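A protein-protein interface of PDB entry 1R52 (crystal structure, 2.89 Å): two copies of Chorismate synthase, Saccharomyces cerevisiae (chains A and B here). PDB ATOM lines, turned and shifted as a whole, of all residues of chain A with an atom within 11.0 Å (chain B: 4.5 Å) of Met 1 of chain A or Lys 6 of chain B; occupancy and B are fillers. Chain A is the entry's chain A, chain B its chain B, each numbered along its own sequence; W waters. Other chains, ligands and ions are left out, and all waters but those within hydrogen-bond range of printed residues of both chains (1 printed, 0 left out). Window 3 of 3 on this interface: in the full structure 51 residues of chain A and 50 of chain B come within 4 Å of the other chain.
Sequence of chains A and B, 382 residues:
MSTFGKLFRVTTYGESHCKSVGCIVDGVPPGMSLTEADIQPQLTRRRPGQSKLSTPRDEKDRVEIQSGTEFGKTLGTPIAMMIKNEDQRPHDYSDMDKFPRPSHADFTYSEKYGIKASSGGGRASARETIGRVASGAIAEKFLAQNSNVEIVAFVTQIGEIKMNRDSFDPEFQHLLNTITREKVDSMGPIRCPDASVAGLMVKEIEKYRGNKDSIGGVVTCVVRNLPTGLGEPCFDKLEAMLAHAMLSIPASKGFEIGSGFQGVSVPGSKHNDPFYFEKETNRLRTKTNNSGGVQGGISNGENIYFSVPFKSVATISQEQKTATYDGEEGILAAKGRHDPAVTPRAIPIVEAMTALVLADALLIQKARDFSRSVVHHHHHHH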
ATOM      1  N   MET A   1      33.665 -29.051 -14.054  1.00  0.00           N
ATOM      2  CA  MET A   1      32.852 -30.266 -13.887  1.00  0.00           C
ATOM      3  C   MET A   1      32.362 -30.680 -15.246  1.00  0.00           C
ATOM      4  O   MET A   1      32.290 -29.863 -16.119  1.00  0.00           O
ATOM      5  CB  MET A   1      31.617 -29.943 -13.019  1.00  0.00           C
ATOM      6  CG  MET A   1      30.818 -31.099 -12.241  1.00  0.00           C
ATOM      7  SD  MET A   1      29.651 -30.331 -10.916  1.00  0.00           S
ATOM      8  CE  MET A   1      30.495 -30.561  -9.433  1.00  0.00           C
ATOM      9  N   SER A   2      32.000 -31.955 -15.386  1.00  0.00           N
ATOM     10  CA  SER A   2      31.327 -32.520 -16.557  1.00  0.00           C
ATOM     11  C   SER A   2      29.896 -32.894 -16.232  1.00  0.00           C
ATOM     12  O   SER A   2      29.177 -33.392 -17.058  1.00  0.00           O
ATOM     13  CB  SER A   2      32.049 -33.787 -17.049  1.00  0.00           C
ATOM     14  OG  SER A   2      33.449 -33.589 -17.095  1.00  0.00           O
ATOM     15  N   THR A   3      29.475 -32.663 -15.022  1.00  0.00           N
ATOM     16  CA  THR A   3      28.101 -32.958 -14.675  1.00  0.00           C
ATOM     17  C   THR A   3      27.329 -31.624 -14.626  1.00  0.00           C
ATOM     18  O   THR A   3      27.822 -30.616 -14.112  1.00  0.00           O
ATOM     19  CB  THR A   3      27.969 -33.774 -13.334  1.00  0.00           C
ATOM     20  OG1 THR A   3      28.495 -35.100 -13.483  1.00  0.00           O
ATOM     21  CG2 THR A   3      26.540 -34.074 -13.048  1.00  0.00           C
ATOM     22  N   PHE A   4      26.151 -31.633 -15.211  1.00  0.00           N
ATOM     23  CA  PHE A   4      25.313 -30.489 -15.232  1.00  0.00           C
ATOM     24  C   PHE A   4      23.935 -30.821 -14.742  1.00  0.00           C
ATOM     25  O   PHE A   4      23.232 -31.674 -15.297  1.00  0.00           O
ATOM     26  CB  PHE A   4      25.203 -29.879 -16.641  1.00  0.00           C
ATOM     27  CG  PHE A   4      24.355 -28.598 -16.695  1.00  0.00           C
ATOM     28  CD1 PHE A   4      24.923 -27.366 -16.449  1.00  0.00           C
ATOM     29  CD2 PHE A   4      22.985 -28.674 -17.006  1.00  0.00           C
ATOM     30  CE1 PHE A   4      24.154 -26.244 -16.486  1.00  0.00           C
ATOM     31  CE2 PHE A   4      22.194 -27.557 -17.082  1.00  0.00           C
ATOM     32  CZ  PHE A   4      22.790 -26.323 -16.793  1.00  0.00           C
ATOM     33  N   GLY A   5      23.560 -30.070 -13.723  1.00  0.00           N
ATOM     34  CA  GLY A   5      22.235 -30.125 -13.171  1.00  0.00           C
ATOM     35  C   GLY A   5      22.190 -30.784 -11.835  1.00  0.00           C
ATOM     36  O   GLY A   5      23.162 -31.405 -11.423  1.00  0.00           O
ATOM     37  N   LYS A   6      21.032 -30.660 -11.202  1.00  0.00           N
ATOM     38  CA  LYS A   6      20.810 -31.116  -9.842  1.00  0.00           C
ATOM     39  C   LYS A   6      20.037 -32.437  -9.741  1.00  0.00           C
ATOM     40  O   LYS A   6      20.493 -33.365  -9.151  1.00  0.00           O
ATOM     41  CB  LYS A   6      20.089 -30.004  -9.065  1.00  0.00           C
ATOM     42  CG  LYS A   6      20.314 -30.088  -7.534  1.00  0.00           C
ATOM     43  CD  LYS A   6      20.196 -28.702  -6.704  1.00  0.00           C
ATOM     44  CE  LYS A   6      19.874 -29.012  -5.155  1.00  0.00           C
ATOM     45  NZ  LYS A   6      20.961 -29.757  -4.280  1.00  0.00           N
ATOM     46  N   PHE A   8      17.899 -33.454 -12.751  1.00  0.00           N
ATOM     47  CA  PHE A   8      18.040 -33.901 -14.132  1.00  0.00           C
ATOM     48  C   PHE A   8      19.497 -33.708 -14.548  1.00  0.00           C
ATOM     49  O   PHE A   8      19.890 -32.619 -14.940  1.00  0.00           O
ATOM     50  CB  PHE A   8      17.124 -33.052 -15.000  1.00  0.00           C
ATOM     51  CG  PHE A   8      16.903 -33.615 -16.358  1.00  0.00           C
ATOM     52  CD1 PHE A   8      15.721 -34.270 -16.666  1.00  0.00           C
ATOM     53  CD2 PHE A   8      17.876 -33.520 -17.343  1.00  0.00           C
ATOM     54  CE1 PHE A   8      15.527 -34.807 -17.936  1.00  0.00           C
ATOM     55  CE2 PHE A   8      17.670 -34.082 -18.596  1.00  0.00           C
ATOM     56  CZ  PHE A   8      16.483 -34.710 -18.880  1.00  0.00           C
ATOM     57  N   ARG A   9      20.323 -34.738 -14.441  1.00  0.00           N
ATOM     58  CA  ARG A   9      21.753 -34.545 -14.554  1.00  0.00           C
ATOM     59  C   ARG A   9      22.237 -35.024 -15.896  1.00  0.00           C
ATOM     60  O   ARG A   9      21.681 -35.928 -16.405  1.00  0.00           O
ATOM     61  CB  ARG A   9      22.477 -35.308 -13.444  1.00  0.00           C
ATOM     62  CG  ARG A   9      22.538 -34.629 -11.988  1.00  0.00           C
ATOM     63  CD  ARG A   9      23.037 -35.564 -10.784  1.00  0.00           C
ATOM     64  NE  ARG A   9      22.197 -36.784 -10.741  1.00  0.00           N
ATOM     65  CZ  ARG A   9      21.062 -37.014  -9.998  1.00  0.00           C
ATOM     66  NH1 ARG A   9      20.539 -36.136  -9.138  1.00  0.00           N
ATOM     67  NH2 ARG A   9      20.452 -38.194 -10.104  1.00  0.00           N
ATOM     68  N   VAL A  10      23.285 -34.410 -16.455  1.00  0.00           N
ATOM     69  CA  VAL A  10      23.983 -34.927 -17.636  1.00  0.00           C
ATOM     70  C   VAL A  10      25.473 -34.897 -17.372  1.00  0.00           C
ATOM     71  O   VAL A  10      25.955 -33.933 -16.876  1.00  0.00           O
ATOM     72  CB  VAL A  10      23.693 -34.130 -18.946  1.00  0.00           C
ATOM     73  CG1 VAL A  10      23.919 -32.660 -18.764  1.00  0.00           C
ATOM     74  CG2 VAL A  10      24.571 -34.591 -20.127  1.00  0.00           C
ATOM     75  N   THR A  11      26.188 -35.969 -17.688  1.00  0.00           N
ATOM     76  CA  THR A  11      27.615 -36.042 -17.482  1.00  0.00           C
ATOM     77  C   THR A  11      28.147 -36.347 -18.845  1.00  0.00           C
ATOM     78  O   THR A  11      27.579 -37.152 -19.509  1.00  0.00           O
ATOM     79  CB  THR A  11      27.964 -37.180 -16.547  1.00  0.00           C
ATOM     80  OG1 THR A  11      27.410 -36.987 -15.226  1.00  0.00           O
ATOM     81  CG2 THR A  11      29.450 -37.217 -16.341  1.00  0.00           C
ATOM     82  N   THR A  12      29.225 -35.727 -19.278  1.00  0.00           N
ATOM     83  CA  THR A  12      29.665 -35.835 -20.652  1.00  0.00           C
ATOM     84  C   THR A  12      31.125 -36.191 -20.699  1.00  0.00           C
ATOM     85  O   THR A  12      31.851 -36.031 -19.732  1.00  0.00           O
ATOM     86  CB  THR A  12      29.477 -34.470 -21.423  1.00  0.00           C
ATOM     87  OG1 THR A  12      29.958 -33.369 -20.629  1.00  0.00           O
ATOM     88  CG2 THR A  12      28.011 -34.139 -21.692  1.00  0.00           C
ATOM     89  N   TYR A  13      31.543 -36.616 -21.891  1.00  0.00           N
ATOM     90  CA  TYR A  13      32.923 -37.058 -22.217  1.00  0.00           C
ATOM     91  C   TYR A  13      33.191 -37.008 -23.689  1.00  0.00           C
ATOM     92  O   TYR A  13      32.331 -37.292 -24.464  1.00  0.00           O
ATOM     93  CB  TYR A  13      33.164 -38.508 -21.835  1.00  0.00           C
ATOM     94  CG  TYR A  13      32.531 -39.548 -22.732  1.00  0.00           C
ATOM     95  CD1 TYR A  13      33.260 -40.205 -23.677  1.00  0.00           C
ATOM     96  CD2 TYR A  13      31.229 -39.923 -22.574  1.00  0.00           C
ATOM     97  CE1 TYR A  13      32.706 -41.183 -24.466  1.00  0.00           C
ATOM     98  CE2 TYR A  13      30.671 -40.893 -23.345  1.00  0.00           C
ATOM     99  CZ  TYR A  13      31.414 -41.522 -24.289  1.00  0.00           C
ATOM    100  OH  TYR A  13      30.841 -42.513 -25.038  1.00  0.00           O
ATOM    101  N   GLY A  14      34.414 -36.714 -24.069  1.00  0.00           N
ATOM    102  CA  GLY A  14      34.743 -36.760 -25.475  1.00  0.00           C
ATOM    103  C   GLY A  14      35.921 -35.917 -25.906  1.00  0.00           C
ATOM    104  O   GLY A  14      35.939 -34.670 -25.716  1.00  0.00           O
ATOM    105  N   GLU A 128      34.024 -30.811 -26.811  1.00  0.00           N
ATOM    106  CA  GLU A 128      32.799 -31.295 -27.439  1.00  0.00           C
ATOM    107  C   GLU A 128      31.453 -31.062 -26.737  1.00  0.00           C
ATOM    108  O   GLU A 128      31.328 -31.228 -25.516  1.00  0.00           O
ATOM    109  CB  GLU A 128      32.898 -32.785 -27.684  1.00  0.00           C
ATOM    110  CG  GLU A 128      32.224 -33.157 -28.982  1.00  0.00           C
ATOM    111  CD  GLU A 128      32.652 -32.230 -30.106  1.00  0.00           C
ATOM    112  OE1 GLU A 128      33.859 -31.874 -30.178  1.00  0.00           O
ATOM    113  OE2 GLU A 128      31.768 -31.828 -30.890  1.00  0.00           O
ATOM    114  N   ARG A 132      25.899 -32.281 -25.156  1.00  0.00           N
ATOM    115  CA  ARG A 132      24.940 -31.291 -24.818  1.00  0.00           C
ATOM    116  C   ARG A 132      23.694 -31.476 -25.643  1.00  0.00           C
ATOM    117  O   ARG A 132      22.590 -31.642 -25.098  1.00  0.00           O
ATOM    118  CB  ARG A 132      25.560 -29.924 -25.068  1.00  0.00           C
ATOM    119  CG  ARG A 132      26.453 -29.565 -23.939  1.00  0.00           C
ATOM    120  CD  ARG A 132      26.867 -28.142 -23.886  1.00  0.00           C
ATOM    121  NE  ARG A 132      28.249 -27.956 -23.402  1.00  0.00           N
ATOM    122  CZ  ARG A 132      28.638 -26.910 -22.682  1.00  0.00           C
ATOM    123  NH1 ARG A 132      27.770 -25.962 -22.322  1.00  0.00           N
ATOM    124  NH2 ARG A 132      29.898 -26.811 -22.305  1.00  0.00           N
ATOM    125  N   PHE A 235      20.074 -17.894  -4.472  1.00  0.00           N
ATOM    126  CA  PHE A 235      21.316 -18.084  -5.209  1.00  0.00           C
ATOM    127  C   PHE A 235      21.123 -18.724  -6.587  1.00  0.00           C
ATOM    128  O   PHE A 235      21.894 -18.471  -7.518  1.00  0.00           O
ATOM    129  CB  PHE A 235      22.365 -18.829  -4.340  1.00  0.00           C
ATOM    130  CG  PHE A 235      23.108 -17.924  -3.384  1.00  0.00           C
ATOM    131  CD1 PHE A 235      23.724 -16.761  -3.821  1.00  0.00           C
ATOM    132  CD2 PHE A 235      23.150 -18.207  -2.035  1.00  0.00           C
ATOM    133  CE1 PHE A 235      24.374 -15.885  -2.934  1.00  0.00           C
ATOM    134  CE2 PHE A 235      23.806 -17.352  -1.129  1.00  0.00           C
ATOM    135  CZ  PHE A 235      24.422 -16.183  -1.596  1.00  0.00           C
ATOM    136  N   ASP A 236      20.076 -19.533  -6.695  1.00  0.00           N
ATOM    137  CA  ASP A 236      19.779 -20.294  -7.887  1.00  0.00           C
ATOM    138  C   ASP A 236      18.528 -19.841  -8.641  1.00  0.00           C
ATOM    139  O   ASP A 236      17.739 -20.611  -9.085  1.00  0.00           O
ATOM    140  CB  ASP A 236      19.739 -21.755  -7.474  1.00  0.00           C
ATOM    141  CG  ASP A 236      21.102 -22.274  -7.167  1.00  0.00           C
ATOM    142  OD1 ASP A 236      22.092 -21.811  -7.739  1.00  0.00           O
ATOM    143  OD2 ASP A 236      21.321 -23.129  -6.341  1.00  0.00           O
ATOM    144  N   MET A 241      20.680 -19.770 -13.372  1.00  0.00           N
ATOM    145  CA  MET A 241      20.874 -21.100 -13.867  1.00  0.00           C
ATOM    146  C   MET A 241      21.062 -20.994 -15.375  1.00  0.00           C
ATOM    147  O   MET A 241      22.010 -21.529 -15.937  1.00  0.00           O
ATOM    148  CB  MET A 241      19.667 -21.982 -13.489  1.00  0.00           C
ATOM    149  CG  MET A 241      19.603 -22.481 -11.984  1.00  0.00           C
ATOM    150  SD  MET A 241      21.136 -22.065 -10.864  1.00  0.00           S
ATOM    151  CE  MET A 241      22.312 -23.603 -11.111  1.00  0.00           C
ATOM    152  N   HIS A 244      24.401 -19.448 -16.234  1.00  0.00           N
ATOM    153  CA  HIS A 244      25.490 -20.406 -16.003  1.00  0.00           C
ATOM    154  C   HIS A 244      25.575 -21.332 -17.226  1.00  0.00           C
ATOM    155  O   HIS A 244      26.678 -21.726 -17.668  1.00  0.00           O
ATOM    156  CB  HIS A 244      25.209 -21.198 -14.725  1.00  0.00           C
ATOM    157  CG  HIS A 244      26.138 -22.344 -14.505  1.00  0.00           C
ATOM    158  ND1 HIS A 244      25.830 -23.621 -14.896  1.00  0.00           N
ATOM    159  CD2 HIS A 244      27.359 -22.418 -13.923  1.00  0.00           C
ATOM    160  CE1 HIS A 244      26.851 -24.424 -14.633  1.00  0.00           C
ATOM    161  NE2 HIS A 244      27.789 -23.723 -14.026  1.00  0.00           N
ATOM    162  N   ALA A 245      24.389 -21.684 -17.743  1.00  0.00           N
ATOM    163  CA  ALA A 245      24.236 -22.638 -18.861  1.00  0.00           C
ATOM    164  C   ALA A 245      24.838 -22.116 -20.164  1.00  0.00           C
ATOM    165  O   ALA A 245      25.569 -22.836 -20.843  1.00  0.00           O
ATOM    166  CB  ALA A 245      22.724 -22.976 -19.094  1.00  0.00           C
ATOM    167  N   SER A 248      28.899 -21.305 -20.300  1.00  0.00           N
ATOM    168  CA  SER A 248      29.661 -22.518 -20.455  1.00  0.00           C
ATOM    169  C   SER A 248      29.717 -22.904 -21.894  1.00  0.00           C
ATOM    170  O   SER A 248      30.558 -23.701 -22.250  1.00  0.00           O
ATOM    171  CB  SER A 248      29.014 -23.709 -19.700  1.00  0.00           C
ATOM    172  OG  SER A 248      27.859 -24.270 -20.378  1.00  0.00           O
ATOM    173  N   ILE A 249      28.836 -22.423 -22.742  1.00  0.00           N
ATOM    174  CA  ILE A 249      28.971 -22.812 -24.137  1.00  0.00           C
ATOM    175  C   ILE A 249      30.265 -22.214 -24.726  1.00  0.00           C
ATOM    176  O   ILE A 249      30.610 -21.030 -24.424  1.00  0.00           O
ATOM    177  CB  ILE A 249      27.803 -22.378 -24.965  1.00  0.00           C
ATOM    178  CG1 ILE A 249      26.512 -22.905 -24.363  1.00  0.00           C
ATOM    179  CG2 ILE A 249      27.956 -22.927 -26.372  1.00  0.00           C
ATOM    180  CD1 ILE A 249      25.287 -22.396 -25.012  1.00  0.00           C
ATOM    181  N   MET A 353      20.859 -26.510 -23.899  1.00  0.00           N
ATOM    182  CA  MET A 353      21.161 -26.032 -22.546  1.00  0.00           C
ATOM    183  C   MET A 353      19.918 -25.412 -21.884  1.00  0.00           C
ATOM    184  O   MET A 353      19.639 -25.635 -20.748  1.00  0.00           O
ATOM    185  CB  MET A 353      22.234 -24.980 -22.651  1.00  0.00           C
ATOM    186  CG  MET A 353      23.589 -25.522 -23.052  1.00  0.00           C
ATOM    187  SD  MET A 353      24.249 -26.568 -21.655  1.00  0.00           S
ATOM    188  CE  MET A 353      24.017 -27.923 -22.322  1.00  0.00           C
ATOM    189  N   ASP A 360      15.453 -29.500 -15.374  1.00  0.00           N
ATOM    190  CA  ASP A 360      15.979 -29.585 -14.010  1.00  0.00           C
ATOM    191  C   ASP A 360      15.090 -28.777 -13.062  1.00  0.00           C
ATOM    192  O   ASP A 360      14.748 -29.242 -12.002  1.00  0.00           O
ATOM    193  CB  ASP A 360      17.415 -29.082 -13.974  1.00  0.00           C
ATOM    194  CG  ASP A 360      18.159 -29.519 -12.753  1.00  0.00           C
ATOM    195  OD1 ASP A 360      17.844 -30.596 -12.198  1.00  0.00           O
ATOM    196  OD2 ASP A 360      19.137 -28.851 -12.312  1.00  0.00           O
ATOM    197  N   GLY B   5      28.300 -22.103  -3.547  1.00  0.00           N
ATOM    198  CA  GLY B   5      29.651 -22.554  -3.651  1.00  0.00           C
ATOM    199  C   GLY B   5      29.785 -24.004  -3.410  1.00  0.00           C
ATOM    200  O   GLY B   5      28.856 -24.596  -2.883  1.00  0.00           O
ATOM    201  N   LYS B   6      30.942 -24.546  -3.783  1.00  0.00           N
ATOM    202  CA  LYS B   6      31.215 -25.973  -3.716  1.00  0.00           C
ATOM    203  C   LYS B   6      32.102 -26.386  -2.514  1.00  0.00           C
ATOM    204  O   LYS B   6      31.773 -27.240  -1.744  1.00  0.00           O
ATOM    205  CB  LYS B   6      31.848 -26.363  -5.054  1.00  0.00           C
ATOM    206  CG  LYS B   6      31.935 -27.895  -5.328  1.00  0.00           C
ATOM    207  CD  LYS B   6      31.869 -28.326  -6.892  1.00  0.00           C
ATOM    208  CE  LYS B   6      32.244 -29.864  -7.067  1.00  0.00           C
ATOM    209  NZ  LYS B   6      31.201 -30.885  -6.544  1.00  0.00           N
ATOM    210  N   LEU B   7      33.263 -25.784  -2.418  1.00  0.00           N
ATOM    211  CA  LEU B   7      34.173 -25.996  -1.294  1.00  0.00           C
ATOM    212  C   LEU B   7      34.163 -24.794  -0.341  1.00  0.00           C
ATOM    213  O   LEU B   7      34.150 -24.985   0.871  1.00  0.00           O
ATOM    214  CB  LEU B   7      35.607 -26.242  -1.781  1.00  0.00           C
ATOM    215  CG  LEU B   7      35.719 -27.451  -2.687  1.00  0.00           C
ATOM    216  CD1 LEU B   7      37.111 -27.481  -3.330  1.00  0.00           C
ATOM    217  CD2 LEU B   7      35.397 -28.737  -1.925  1.00  0.00           C
ATOM    218  N   PHE B   8      34.140 -23.583  -0.890  1.00  0.00           N
ATOM    219  CA  PHE B   8      33.979 -22.381  -0.072  1.00  0.00           C
ATOM    220  C   PHE B   8      32.498 -22.014  -0.030  1.00  0.00           C
ATOM    221  O   PHE B   8      32.017 -21.354  -0.937  1.00  0.00           O
ATOM    222  CB  PHE B   8      34.808 -21.259  -0.704  1.00  0.00           C
ATOM    223  CG  PHE B   8      35.049 -20.118   0.200  1.00  0.00           C
ATOM    224  CD1 PHE B   8      36.268 -19.950   0.834  1.00  0.00           C
ATOM    225  CD2 PHE B   8      34.065 -19.193   0.457  1.00  0.00           C
ATOM    226  CE1 PHE B   8      36.487 -18.830   1.706  1.00  0.00           C
ATOM    227  CE2 PHE B   8      34.293 -18.101   1.326  1.00  0.00           C
ATOM    228  CZ  PHE B   8      35.514 -17.944   1.928  1.00  0.00           C
ATOM    229  N   ARG B   9      31.744 -22.440   0.963  1.00  0.00           N
ATOM    230  CA  ARG B   9      30.284 -22.357   0.846  1.00  0.00           C
ATOM    231  C   ARG B   9      29.791 -21.229   1.697  1.00  0.00           C
ATOM    232  O   ARG B   9      30.419 -20.934   2.678  1.00  0.00           O
ATOM    233  CB  ARG B   9      29.558 -23.666   1.292  1.00  0.00           C
ATOM    234  CG  ARG B   9      29.639 -24.923   0.336  1.00  0.00           C
ATOM    235  CD  ARG B   9      29.253 -26.307   0.976  1.00  0.00           C
ATOM    236  NE  ARG B   9      30.216 -26.631   2.049  1.00  0.00           N
ATOM    237  CZ  ARG B   9      31.363 -27.407   1.991  1.00  0.00           C
ATOM    238  NH1 ARG B   9      31.797 -28.056   0.894  1.00  0.00           N
ATOM    239  NH2 ARG B   9      32.091 -27.533   3.107  1.00  0.00           N
ATOM    240  N   GLU B 232      36.795 -24.792 -14.174  1.00  0.00           N
ATOM    241  CA  GLU B 232      36.506 -26.237 -14.242  1.00  0.00           C
ATOM    242  C   GLU B 232      35.873 -26.656 -15.583  1.00  0.00           C
ATOM    243  O   GLU B 232      34.731 -27.105 -15.594  1.00  0.00           O
ATOM    244  CB  GLU B 232      35.545 -26.579 -13.086  1.00  0.00           C
ATOM    245  CG  GLU B 232      36.190 -26.641 -11.710  1.00  0.00           C
ATOM    246  CD  GLU B 232      37.211 -27.771 -11.610  1.00  0.00           C
ATOM    247  OE1 GLU B 232      36.794 -28.943 -11.931  1.00  0.00           O
ATOM    248  OE2 GLU B 232      38.407 -27.495 -11.227  1.00  0.00           O
ATOM    249  N   PRO B 233      36.597 -26.465 -16.692  1.00  0.00           N
ATOM    250  CA  PRO B 233      36.063 -26.591 -18.069  1.00  0.00           C
ATOM    251  C   PRO B 233      35.082 -27.748 -18.331  1.00  0.00           C
ATOM    252  O   PRO B 233      35.072 -28.814 -17.694  1.00  0.00           O
ATOM    253  CB  PRO B 233      37.317 -26.780 -18.942  1.00  0.00           C
ATOM    254  CG  PRO B 233      38.384 -27.008 -17.949  1.00  0.00           C
ATOM    255  CD  PRO B 233      38.004 -26.121 -16.739  1.00  0.00           C
ATOM    256  N   CYS B 234      34.304 -27.492 -19.371  1.00  0.00           N
ATOM    257  CA  CYS B 234      33.081 -28.203 -19.658  1.00  0.00           C
ATOM    258  C   CYS B 234      31.936 -27.375 -19.110  1.00  0.00           C
ATOM    259  O   CYS B 234      31.492 -26.445 -19.772  1.00  0.00           O
ATOM    260  CB  CYS B 234      33.056 -29.644 -19.096  1.00  0.00           C
ATOM    261  SG  CYS B 234      34.007 -30.841 -20.100  1.00  0.00           S
ATOM    262  N   PHE B 235      31.455 -27.671 -17.918  1.00  0.00           N
ATOM    263  CA  PHE B 235      30.207 -27.056 -17.483  1.00  0.00           C
ATOM    264  C   PHE B 235      30.377 -25.883 -16.516  1.00  0.00           C
ATOM    265  O   PHE B 235      29.543 -24.966 -16.479  1.00  0.00           O
ATOM    266  CB  PHE B 235      29.231 -28.117 -16.927  1.00  0.00           C
ATOM    267  CG  PHE B 235      28.507 -28.865 -17.997  1.00  0.00           C
ATOM    268  CD1 PHE B 235      27.830 -28.192 -19.005  1.00  0.00           C
ATOM    269  CD2 PHE B 235      28.545 -30.237 -18.045  1.00  0.00           C
ATOM    270  CE1 PHE B 235      27.179 -28.869 -20.036  1.00  0.00           C
ATOM    271  CE2 PHE B 235      27.891 -30.946 -19.073  1.00  0.00           C
ATOM    272  CZ  PHE B 235      27.198 -30.231 -20.075  1.00  0.00           C
ATOM    273  N   ASP B 236      31.459 -25.927 -15.746  1.00  0.00           N
ATOM    274  CA  ASP B 236      31.723 -24.949 -14.713  1.00  0.00           C
ATOM    275  C   ASP B 236      32.924 -24.100 -14.977  1.00  0.00           C
ATOM    276  O   ASP B 236      33.723 -23.875 -14.124  1.00  0.00           O
ATOM    277  CB  ASP B 236      31.826 -25.672 -13.384  1.00  0.00           C
ATOM    278  CG  ASP B 236      30.488 -26.202 -12.930  1.00  0.00           C
ATOM    279  OD1 ASP B 236      29.444 -25.561 -13.166  1.00  0.00           O
ATOM    280  OD2 ASP B 236      30.375 -27.262 -12.338  1.00  0.00           O
ATOM    281  N   ASP B 360      36.279 -19.892  -4.079  1.00  0.00           N
ATOM    282  CA  ASP B 360      35.809 -21.236  -4.325  1.00  0.00           C
ATOM    283  C   ASP B 360      36.682 -21.892  -5.379  1.00  0.00           C
ATOM    284  O   ASP B 360      37.123 -23.024  -5.217  1.00  0.00           O
ATOM    285  CB  ASP B 360      34.363 -21.208  -4.760  1.00  0.00           C
ATOM    286  CG  ASP B 360      33.666 -22.555  -4.599  1.00  0.00           C
ATOM    287  OD1 ASP B 360      34.050 -23.394  -3.750  1.00  0.00           O
ATOM    288  OD2 ASP B 360      32.655 -22.854  -5.290  1.00  0.00           O
ATOM    289  N   ILE B 364      39.164 -25.310  -5.277  1.00  0.00           N
ATOM    290  CA  ILE B 364      38.994 -26.409  -6.249  1.00  0.00           C
ATOM    291  C   ILE B 364      40.206 -26.594  -7.123  1.00  0.00           C
ATOM    292  O   ILE B 364      40.456 -27.659  -7.664  1.00  0.00           O
ATOM    293  CB  ILE B 364      37.793 -26.186  -7.169  1.00  0.00           C
ATOM    294  CG1 ILE B 364      36.558 -25.708  -6.417  1.00  0.00           C
ATOM    295  CG2 ILE B 364      37.408 -27.452  -7.851  1.00  0.00           C
ATOM    296  CD1 ILE B 364      35.260 -25.609  -7.285  1.00  0.00           C
HETATM  297  O   HOH W   1      27.506 -27.419 -13.955  1.00  0.00           O
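O of Pro 233 of chain B sits close to O of Met 1 of chain A.
The side-chain carboxylate (OD1) of Asp 236 of chain B lies within hydrogen-bond range of a ring nitrogen (NE2) of His 244 of chain A, at 2.6 Å.
The backbone carbonyl oxygen (O) of Met 1 of chain A is in hydrogen-bond range of the backbone NH (N) of Phe 235 of chain B, 3.0 Å away.
The backbone carbonyl oxygen (O) of Phe 235 of chain B sits at hydrogen-bond distance from a ring nitrogen (NE2) of His 244 of chain A.
SD of Met 1 of chain A lies close to OD2 of Asp 236 of chain B (3.5 Å).
The backbone carbonyl oxygen of Glu 232 of chain B sits at hydrogen-bond distance from the backbone NH of Met 1 of chain A (2.7 Å).
The backbone carbonyl oxygen (O) of Cys 234 of chain B sits at hydrogen-bond distance from the guanidinium group (NH2) of Arg 132 of chain A (3.0 Å).
The side-chain sulfur (SD) of Met 353 of chain A lies within hydrogen-bond range of the guanidinium group (NH1) of Arg 132 of chain A, at 3.6 Å.
The guanidinium group (NH1) of Arg 132 of chain A lies within hydrogen-bond range of the side-chain hydroxyl (OG) of Ser 248 of chain A, at 2.6 Å.
The backbone carbonyl oxygen (O) of Ser 2 of chain A is in hydrogen-bond range of the backbone NH (N) of Thr 12 of chain A (3.2 Å).
OG1 of Thr 11 of chain A is in hydrogen-bond range of OG1 of Thr 3 of chain A (2.8 Å).
Among the printed residues, merely in contact across the chains: Met 1 of chain A with Lys 6 of chain B, Met 1 of chain A with Cys 234 of chain B, Ser 2 of chain A with Phe 235 of chain B, Thr 3 of chain A with Phe 235 of chain B, Phe 4 of chain A with Phe 235 of chain B, Thr 12 of chain A with Phe 235 of chain B, Arg 132 of chain A with Phe 235 of chain B, Ser 248 of chain A with Cys 234 of chain B and Ser 248 of chain A with Phe 235 of chain B.
Of the printed residues of chain B, Ser 2 of chain A touches Phe 235.
Of the printed residues of chain B, Phe 4 of chain A touches Phe 235.
Gly 14 of chain A touches none of the printed residues of chain B.
Printed residues of chain B within 4 Å of Arg 132 of chain A: Cys 234 and Phe 235.
No residue of chain A comes within 4 Å of Gly 5 of chain B.
No residue of chain A comes within 4 Å of Leu 7 of chain B.
Cys 234 of chain B touches just these residues of chain A: Met 1 (3.1 Å), Arg 132 (3.0 Å) and Ser 248 (3.7 Å).
Of chain A, only Met 1 (3.0 Å) and His 244 (2.6 Å) come within 4 Å of Asp 236 of chain B.
Ile 364 of chain B touches none of the printed residues of chain A.
The nearest residue of chain A that does not touch Lys 6 of chain B is Thr 3 of chain A (8.1 Å).
The nearest printed residue of chain B that does not touch His 244 of chain A is Cys 234 of chain B (7.1 Å).
Positions printed for both chains: 5, 6, 8, 9, 235, 236 and 360.
Of the 16 pairs that touch across the chains among the printed residues, none has its exchanged pair printed and touching as well.
Water W1 lies within hydrogen-bond range of the side-chain carboxylate of Asp 236 of chain B (2.8 Å) and the backbone carbonyl oxygen of Thr 3 of chain A (3.2 Å).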
